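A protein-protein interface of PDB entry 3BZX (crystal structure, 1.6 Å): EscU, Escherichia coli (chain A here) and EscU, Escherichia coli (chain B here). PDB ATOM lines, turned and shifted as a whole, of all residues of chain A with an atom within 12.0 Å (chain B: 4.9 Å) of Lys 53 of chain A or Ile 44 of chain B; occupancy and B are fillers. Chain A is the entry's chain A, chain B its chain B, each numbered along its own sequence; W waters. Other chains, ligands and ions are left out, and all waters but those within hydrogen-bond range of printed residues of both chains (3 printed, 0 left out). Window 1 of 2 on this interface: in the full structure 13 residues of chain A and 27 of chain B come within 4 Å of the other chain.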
ATOM      1  N   ILE A  45      11.976 -24.661 -24.610  1.00  0.00           N
ATOM      2  CA  ILE A  45      11.900 -24.820 -23.154  1.00  0.00           C
ATOM      3  C   ILE A  45      11.709 -26.309 -22.814  1.00  0.00           C
ATOM      4  O   ILE A  45      12.342 -26.811 -21.915  1.00  0.00           O
ATOM      5  CB  ILE A  45      10.756 -23.977 -22.522  1.00  0.00           C
ATOM      6  CG1 ILE A  45      10.892 -22.493 -22.871  1.00  0.00           C
ATOM      7  CG2 ILE A  45      10.747 -24.229 -20.959  1.00  0.00           C
ATOM      8  CD1 ILE A  45      12.238 -21.908 -22.596  1.00  0.00           C
ATOM      9  N   SER A  48      14.952 -28.092 -22.751  1.00  0.00           N
ATOM     10  CA  SER A  48      15.945 -27.396 -21.898  1.00  0.00           C
ATOM     11  C   SER A  48      16.470 -28.306 -20.770  1.00  0.00           C
ATOM     12  O   SER A  48      15.812 -29.282 -20.383  1.00  0.00           O
ATOM     13  CB  SER A  48      15.337 -26.126 -21.247  1.00  0.00           C
ATOM     14  OG  SER A  48      15.304 -24.969 -22.101  1.00  0.00           O
ATOM     15  N   THR A  49      17.646 -27.969 -20.249  1.00  0.00           N
ATOM     16  CA  THR A  49      18.209 -28.657 -19.123  1.00  0.00           C
ATOM     17  C   THR A  49      17.921 -27.921 -17.812  1.00  0.00           C
ATOM     18  O   THR A  49      17.528 -28.537 -16.808  1.00  0.00           O
ATOM     19  CB  THR A  49      19.723 -28.837 -19.349  1.00  0.00           C
ATOM     20  OG1 THR A  49      19.956 -29.410 -20.648  1.00  0.00           O
ATOM     21  CG2 THR A  49      20.334 -29.683 -18.239  1.00  0.00           C
ATOM     22  N   VAL A  50      18.079 -26.588 -17.829  1.00  0.00           N
ATOM     23  CA  VAL A  50      17.916 -25.790 -16.634  1.00  0.00           C
ATOM     24  C   VAL A  50      17.682 -24.326 -17.025  1.00  0.00           C
ATOM     25  O   VAL A  50      18.192 -23.875 -18.038  1.00  0.00           O
ATOM     26  CB  VAL A  50      19.146 -25.953 -15.677  1.00  0.00           C
ATOM     27  CG1 VAL A  50      20.422 -25.429 -16.344  1.00  0.00           C
ATOM     28  CG2 VAL A  50      18.906 -25.261 -14.344  1.00  0.00           C
ATOM     29  N   ILE A  51      16.862 -23.646 -16.227  1.00  0.00           N
ATOM     30  CA  ILE A  51      16.539 -22.215 -16.381  1.00  0.00           C
ATOM     31  C   ILE A  51      17.174 -21.469 -15.227  1.00  0.00           C
ATOM     32  O   ILE A  51      16.989 -21.882 -14.085  1.00  0.00           O
ATOM     33  CB  ILE A  51      15.003 -21.916 -16.264  1.00  0.00           C
ATOM     34  CG1 ILE A  51      14.169 -22.919 -17.058  1.00  0.00           C
ATOM     35  CG2 ILE A  51      14.697 -20.518 -16.731  1.00  0.00           C
ATOM     36  CD1 ILE A  51      14.697 -23.141 -18.461  1.00  0.00           C
ATOM     37  N   VAL A  52      17.915 -20.396 -15.511  1.00  0.00           N
ATOM     38  CA  VAL A  52      18.395 -19.478 -14.461  1.00  0.00           C
ATOM     39  C   VAL A  52      17.621 -18.194 -14.563  1.00  0.00           C
ATOM     40  O   VAL A  52      17.423 -17.672 -15.671  1.00  0.00           O
ATOM     41  CB  VAL A  52      19.882 -19.139 -14.620  1.00  0.00           C
ATOM     42  CG1 VAL A  52      20.413 -18.570 -13.290  1.00  0.00           C
ATOM     43  CG2 VAL A  52      20.610 -20.363 -14.994  1.00  0.00           C
ATOM     44  N   LYS A  53      17.096 -17.742 -13.420  1.00  0.00           N
ATOM     45  CA  LYS A  53      16.346 -16.508 -13.343  1.00  0.00           C
ATOM     46  C   LYS A  53      16.909 -15.571 -12.286  1.00  0.00           C
ATOM     47  O   LYS A  53      17.676 -15.971 -11.430  1.00  0.00           O
ATOM     48  CB  LYS A  53      14.863 -16.785 -13.030  1.00  0.00           C
ATOM     49  CG  LYS A  53      14.577 -17.359 -11.658  1.00  0.00           C
ATOM     50  CD  LYS A  53      13.078 -17.593 -11.462  1.00  0.00           C
ATOM     51  CE  LYS A  53      12.342 -16.278 -11.247  1.00  0.00           C
ATOM     52  NZ  LYS A  53      12.660 -15.646  -9.936  1.00  0.00           N
ATOM     53  N   ASN A  54      16.566 -14.304 -12.414  1.00  0.00           N
ATOM     54  CA  ASN A  54      16.823 -13.301 -11.368  1.00  0.00           C
ATOM     55  C   ASN A  54      15.596 -13.170 -10.471  1.00  0.00           C
ATOM     56  O   ASN A  54      14.786 -14.124 -10.470  1.00  0.00           O
ATOM     57  CB  ASN A  54      17.233 -11.960 -11.979  1.00  0.00           C
ATOM     58  CG  ASN A  54      16.086 -11.231 -12.642  1.00  0.00           C
ATOM     59  OD1 ASN A  54      15.089 -11.854 -13.013  1.00  0.00           O
ATOM     60  ND2 ASN A  54      16.238  -9.910 -12.819  1.00  0.00           N
ATOM     61  OXT ASN A  54      15.378 -12.150  -9.793  1.00  0.00           O
ATOM     62  N   ILE B   4      14.405 -11.548 -15.720  1.00  0.00           N
ATOM     63  CA  ILE B   4      15.321 -12.193 -16.675  1.00  0.00           C
ATOM     64  C   ILE B   4      15.182 -13.707 -16.518  1.00  0.00           C
ATOM     65  O   ILE B   4      15.056 -14.195 -15.399  1.00  0.00           O
ATOM     66  CB  ILE B   4      16.814 -11.785 -16.385  1.00  0.00           C
ATOM     67  CG1 ILE B   4      17.093 -10.352 -16.876  1.00  0.00           C
ATOM     68  CG2 ILE B   4      17.827 -12.800 -16.991  1.00  0.00           C
ATOM     69  CD1 ILE B   4      18.427  -9.747 -16.311  1.00  0.00           C
ATOM     70  N   ALA B   5      15.202 -14.418 -17.644  1.00  0.00           N
ATOM     71  CA  ALA B   5      15.273 -15.884 -17.642  1.00  0.00           C
ATOM     72  C   ALA B   5      16.212 -16.341 -18.763  1.00  0.00           C
ATOM     73  O   ALA B   5      16.127 -15.848 -19.892  1.00  0.00           O
ATOM     74  CB  ALA B   5      13.897 -16.530 -17.809  1.00  0.00           C
ATOM     75  N   ILE B  33       9.237 -18.879 -17.674  1.00  0.00           N
ATOM     76  CA  ILE B  33       9.132 -19.561 -16.383  1.00  0.00           C
ATOM     77  C   ILE B  33       7.811 -20.359 -16.278  1.00  0.00           C
ATOM     78  O   ILE B  33       7.809 -21.474 -15.742  1.00  0.00           O
ATOM     79  CB  ILE B  33       9.408 -18.605 -15.199  1.00  0.00           C
ATOM     80  CG1 ILE B  33      10.793 -17.956 -15.363  1.00  0.00           C
ATOM     81  CG2 ILE B  33       9.355 -19.362 -13.888  1.00  0.00           C
ATOM     82  CD1 ILE B  33      11.010 -16.714 -14.464  1.00  0.00           C
ATOM     83  N   PRO B  42      13.883 -27.686 -14.299  1.00  0.00           N
ATOM     84  CA  PRO B  42      14.345 -27.022 -13.096  1.00  0.00           C
ATOM     85  C   PRO B  42      14.618 -25.529 -13.320  1.00  0.00           C
ATOM     86  O   PRO B  42      15.273 -25.155 -14.297  1.00  0.00           O
ATOM     87  CB  PRO B  42      15.635 -27.778 -12.746  1.00  0.00           C
ATOM     88  CG  PRO B  42      15.377 -29.142 -13.264  1.00  0.00           C
ATOM     89  CD  PRO B  42      14.685 -28.905 -14.569  1.00  0.00           C
ATOM     90  N   VAL B  43      14.138 -24.714 -12.379  1.00  0.00           N
ATOM     91  CA  VAL B  43      14.358 -23.270 -12.406  1.00  0.00           C
ATOM     92  C   VAL B  43      15.157 -22.894 -11.153  1.00  0.00           C
ATOM     93  O   VAL B  43      14.758 -23.219 -10.036  1.00  0.00           O
ATOM     94  CB  VAL B  43      13.037 -22.499 -12.443  1.00  0.00           C
ATOM     95  CG1 VAL B  43      13.290 -20.993 -12.288  1.00  0.00           C
ATOM     96  CG2 VAL B  43      12.271 -22.811 -13.738  1.00  0.00           C
ATOM     97  N   ILE B  44      16.295 -22.241 -11.359  1.00  0.00           N
ATOM     98  CA  ILE B  44      17.139 -21.803 -10.256  1.00  0.00           C
ATOM     99  C   ILE B  44      17.261 -20.276 -10.253  1.00  0.00           C
ATOM    100  O   ILE B  44      17.566 -19.662 -11.280  1.00  0.00           O
ATOM    101  CB  ILE B  44      18.547 -22.429 -10.327  1.00  0.00           C
ATOM    102  CG1 ILE B  44      18.459 -23.929 -10.651  1.00  0.00           C
ATOM    103  CG2 ILE B  44      19.287 -22.192  -9.034  1.00  0.00           C
ATOM    104  CD1 ILE B  44      17.576 -24.710  -9.722  1.00  0.00           C
ATOM    105  N   GLU B  45      17.006 -19.676  -9.095  1.00  0.00           N
ATOM    106  CA  GLU B  45      17.189 -18.231  -8.938  1.00  0.00           C
ATOM    107  C   GLU B  45      18.622 -17.943  -8.506  1.00  0.00           C
ATOM    108  O   GLU B  45      19.084 -18.408  -7.430  1.00  0.00           O
ATOM    109  CB  GLU B  45      16.192 -17.649  -7.924  1.00  0.00           C
ATOM    110  CG  GLU B  45      16.380 -16.154  -7.723  1.00  0.00           C
ATOM    111  CD  GLU B  45      15.371 -15.516  -6.775  1.00  0.00           C
ATOM    112  OE1 GLU B  45      14.167 -15.798  -6.907  1.00  0.00           O
ATOM    113  OE2 GLU B  45      15.779 -14.713  -5.930  1.00  0.00           O
ATOM    114  N   ASP B  46      19.334 -17.196  -9.347  1.00  0.00           N
ATOM    115  CA  ASP B  46      20.695 -16.819  -9.060  1.00  0.00           C
ATOM    116  C   ASP B  46      20.890 -15.494  -9.771  1.00  0.00           C
ATOM    117  O   ASP B  46      21.104 -15.431 -10.986  1.00  0.00           O
ATOM    118  CB  ASP B  46      21.699 -17.875  -9.502  1.00  0.00           C
ATOM    119  CG  ASP B  46      23.136 -17.531  -9.104  1.00  0.00           C
ATOM    120  OD1 ASP B  46      23.489 -16.327  -9.097  1.00  0.00           O
ATOM    121  OD2 ASP B  46      23.920 -18.499  -8.816  1.00  0.00           O
ATOM    122  N   ILE B  47      20.723 -14.431  -9.007  1.00  0.00           N
ATOM    123  CA  ILE B  47      20.571 -13.118  -9.619  1.00  0.00           C
ATOM    124  C   ILE B  47      21.874 -12.644 -10.278  1.00  0.00           C
ATOM    125  O   ILE B  47      21.833 -12.210 -11.423  1.00  0.00           O
ATOM    126  CB  ILE B  47      20.000 -12.123  -8.604  1.00  0.00           C
ATOM    127  CG1 ILE B  47      18.562 -12.523  -8.225  1.00  0.00           C
ATOM    128  CG2 ILE B  47      20.079 -10.709  -9.144  1.00  0.00           C
ATOM    129  CD1 ILE B  47      18.022 -11.892  -6.935  1.00  0.00           C
ATOM    130  N   ALA B  50      22.315 -14.900 -13.462  1.00  0.00           N
ATOM    131  CA  ALA B  50      21.323 -14.602 -14.508  1.00  0.00           C
ATOM    132  C   ALA B  50      21.681 -13.308 -15.242  1.00  0.00           C
ATOM    133  O   ALA B  50      21.643 -13.229 -16.457  1.00  0.00           O
ATOM    134  CB  ALA B  50      19.928 -14.461 -13.890  1.00  0.00           C
ATOM    135  N   LEU B  74      24.933 -25.941 -11.981  1.00  0.00           N
ATOM    136  CA  LEU B  74      23.485 -25.970 -12.272  1.00  0.00           C
ATOM    137  C   LEU B  74      23.118 -27.272 -12.978  1.00  0.00           C
ATOM    138  O   LEU B  74      22.088 -27.865 -12.696  1.00  0.00           O
ATOM    139  CB  LEU B  74      23.063 -24.812 -13.179  1.00  0.00           C
ATOM    140  CG  LEU B  74      23.254 -23.360 -12.733  1.00  0.00           C
ATOM    141  CD1 LEU B  74      22.937 -22.426 -13.925  1.00  0.00           C
ATOM    142  CD2 LEU B  74      22.392 -23.073 -11.573  1.00  0.00           C
ATOM    143  N   ILE B  77      22.888 -30.191 -10.582  1.00  0.00           N
ATOM    144  CA  ILE B  77      21.649 -30.127  -9.790  1.00  0.00           C
ATOM    145  C   ILE B  77      20.412 -30.528 -10.597  1.00  0.00           C
ATOM    146  O   ILE B  77      19.439 -31.084 -10.065  1.00  0.00           O
ATOM    147  CB  ILE B  77      21.416 -28.683  -9.242  1.00  0.00           C
ATOM    148  CG1 ILE B  77      22.418 -28.393  -8.115  1.00  0.00           C
ATOM    149  CG2 ILE B  77      19.974 -28.504  -8.765  1.00  0.00           C
ATOM    150  CD1 ILE B  77      22.518 -26.924  -7.761  1.00  0.00           C
HETATM  151  O   HOH W   1      14.009 -12.506  -7.603  1.00  0.00           O
HETATM  152  O   HOH W   2      12.583 -17.569  -8.095  1.00  0.00           O
HETATM  153  O   HOH W   3      12.729 -13.683 -13.487  1.00  0.00           O
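Water W1 bridges the chain-end carboxylate (OXT) of Asn 54 of chain A (2.6 Å) and the side-chain carboxylate (OE2) of Glu 45 of chain B (3.3 Å).
Water W2 lies within hydrogen-bond range of the side-chain carboxylate of Glu 45 of chain B (2.7 Å) and the side-chain amino group of Lys 53 of chain A (2.7 Å).
Water W3 bridges the side-chain amide oxygen of Asn 54 of chain A (3.0 Å) and the backbone carbonyl oxygen of Ile 4 of chain B (3.1 Å).
Among the printed residues, merely in contact across the chains: Val 52 of chain A with Leu 74 of chain B (3.3 Å), Val 52 of chain A with Ile 44 of chain B (3.3 Å), Lys 53 of chain A with Ile 4 of chain B (3.4 Å), Ile 51 of chain A with Val 43 of chain B (3.4 Å), Val 52 of chain A with Ala 5 of chain B (3.4 Å), Lys 53 of chain A with Val 43 of chain B (3.5 Å), Lys 53 of chain A with Ile 33 of chain B (3.5 Å), Asn 54 of chain A with Ile 47 of chain B (3.6 Å), Val 50 of chain A with Pro 42 of chain B (3.6 Å), Lys 53 of chain A with Ala 50 of chain B (3.6 Å), Thr 49 of chain A with Pro 42 of chain B (3.6 Å), Asn 54 of chain A with Ala 50 of chain B (3.7 Å), Asn 54 of chain A with Glu 45 of chain B (3.8 Å), Val 50 of chain A with Ile 44 of chain B (3.95 Å) and Val 52 of chain A with Asp 46 of chain B (3.95 Å).
N of Ile 51 of chain A is in hydrogen-bond range of O of Pro 42 of chain B, at 2.9 Å.
The backbone carbonyl oxygen (O) of Ile 51 of chain A lies within hydrogen-bond range of the backbone NH (N) of Ile 44 of chain B (2.8 Å).
The backbone NH (N) of Lys 53 of chain A lies within hydrogen-bond range of the backbone carbonyl oxygen (O) of Ile 44 of chain B.
The side-chain carboxylate (OE1) of Glu 45 of chain B lies within salt-bridge range of the side-chain amino group (NZ) of Lys 53 of chain A (3.4 Å).
The backbone carbonyl oxygen (O) of Lys 53 of chain A sits at hydrogen-bond distance from the backbone NH (N) of Asp 46 of chain B, at 2.9 Å.
N of Ile 4 of chain B sits at hydrogen-bond distance from OD1 of Asn 54 of chain A (2.8 Å).
Of the printed residues of chain B, Lys 53 of chain A touches Ile 4 (3.4 Å), Ile 33 (3.5 Å), Val 43 (3.5 Å), Ile 44 (2.9 Å), Glu 45 (3.4 Å), Asp 46 (2.9 Å) and Ala 50 (3.6 Å).
Printed residues of chain A within 4 Å of Glu 45 of chain B: Lys 53 (3.4 Å) and Asn 54 (3.8 Å).
Of chain A, only Val 52 and Lys 53 come within 4 Å of Asp 46 of chain B.
Of chain A, only Asn 54 (3.6 Å) comes within 4 Å of Ile 47 of chain B.
Of chain A, only Lys 53 and Asn 54 come within 4 Å of Ala 50 of chain B.
No residue of chain A comes within 4 Å of Ile 77 of chain B.
Of the printed residues of chain B, Val 52 of chain A touches Ala 5 (3.4 Å), Ile 44 (3.3 Å), Asp 46 (3.95 Å) and Leu 74 (3.3 Å).
Of the printed residues of chain B, Val 50 of chain A touches Pro 42 (3.6 Å) and Ile 44 (3.95 Å).
Of the printed residues of chain B, Thr 49 of chain A touches Pro 42 (3.6 Å).
Of the printed residues of chain A, Ile 4 of chain B touches Lys 53 and Asn 54.
Ile 45 of chain A touches none of the printed residues of chain B.
The nearest printed residue of chain B that does not touch Lys 53 of chain A is Ile 47 of chain B (4.2 Å).
The nearest printed residue of chain A that does not touch Ile 44 of chain B is Asn 54 of chain A (5.6 Å).
Hydrophobic or aromatic side chains of chain A that line the printed part of chain B: Val 50, Ile 51 and Val 52.
Of the 12 printed residues of chain B, 11 touch a printed residue of chain A.
Printed residues of chain B that touch a printed residue of chain A: Ile 4, Ala 5, Ile 33, Pro 42, Val 43, Ile 44, Glu 45, Asp 46, Ile 47, Ala 50 and Leu 74.
Along chain B the printed residues that touch a printed residue of chain A span positions 4 to 74.
Among the printed residues, 21 pairs touch across the chains.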
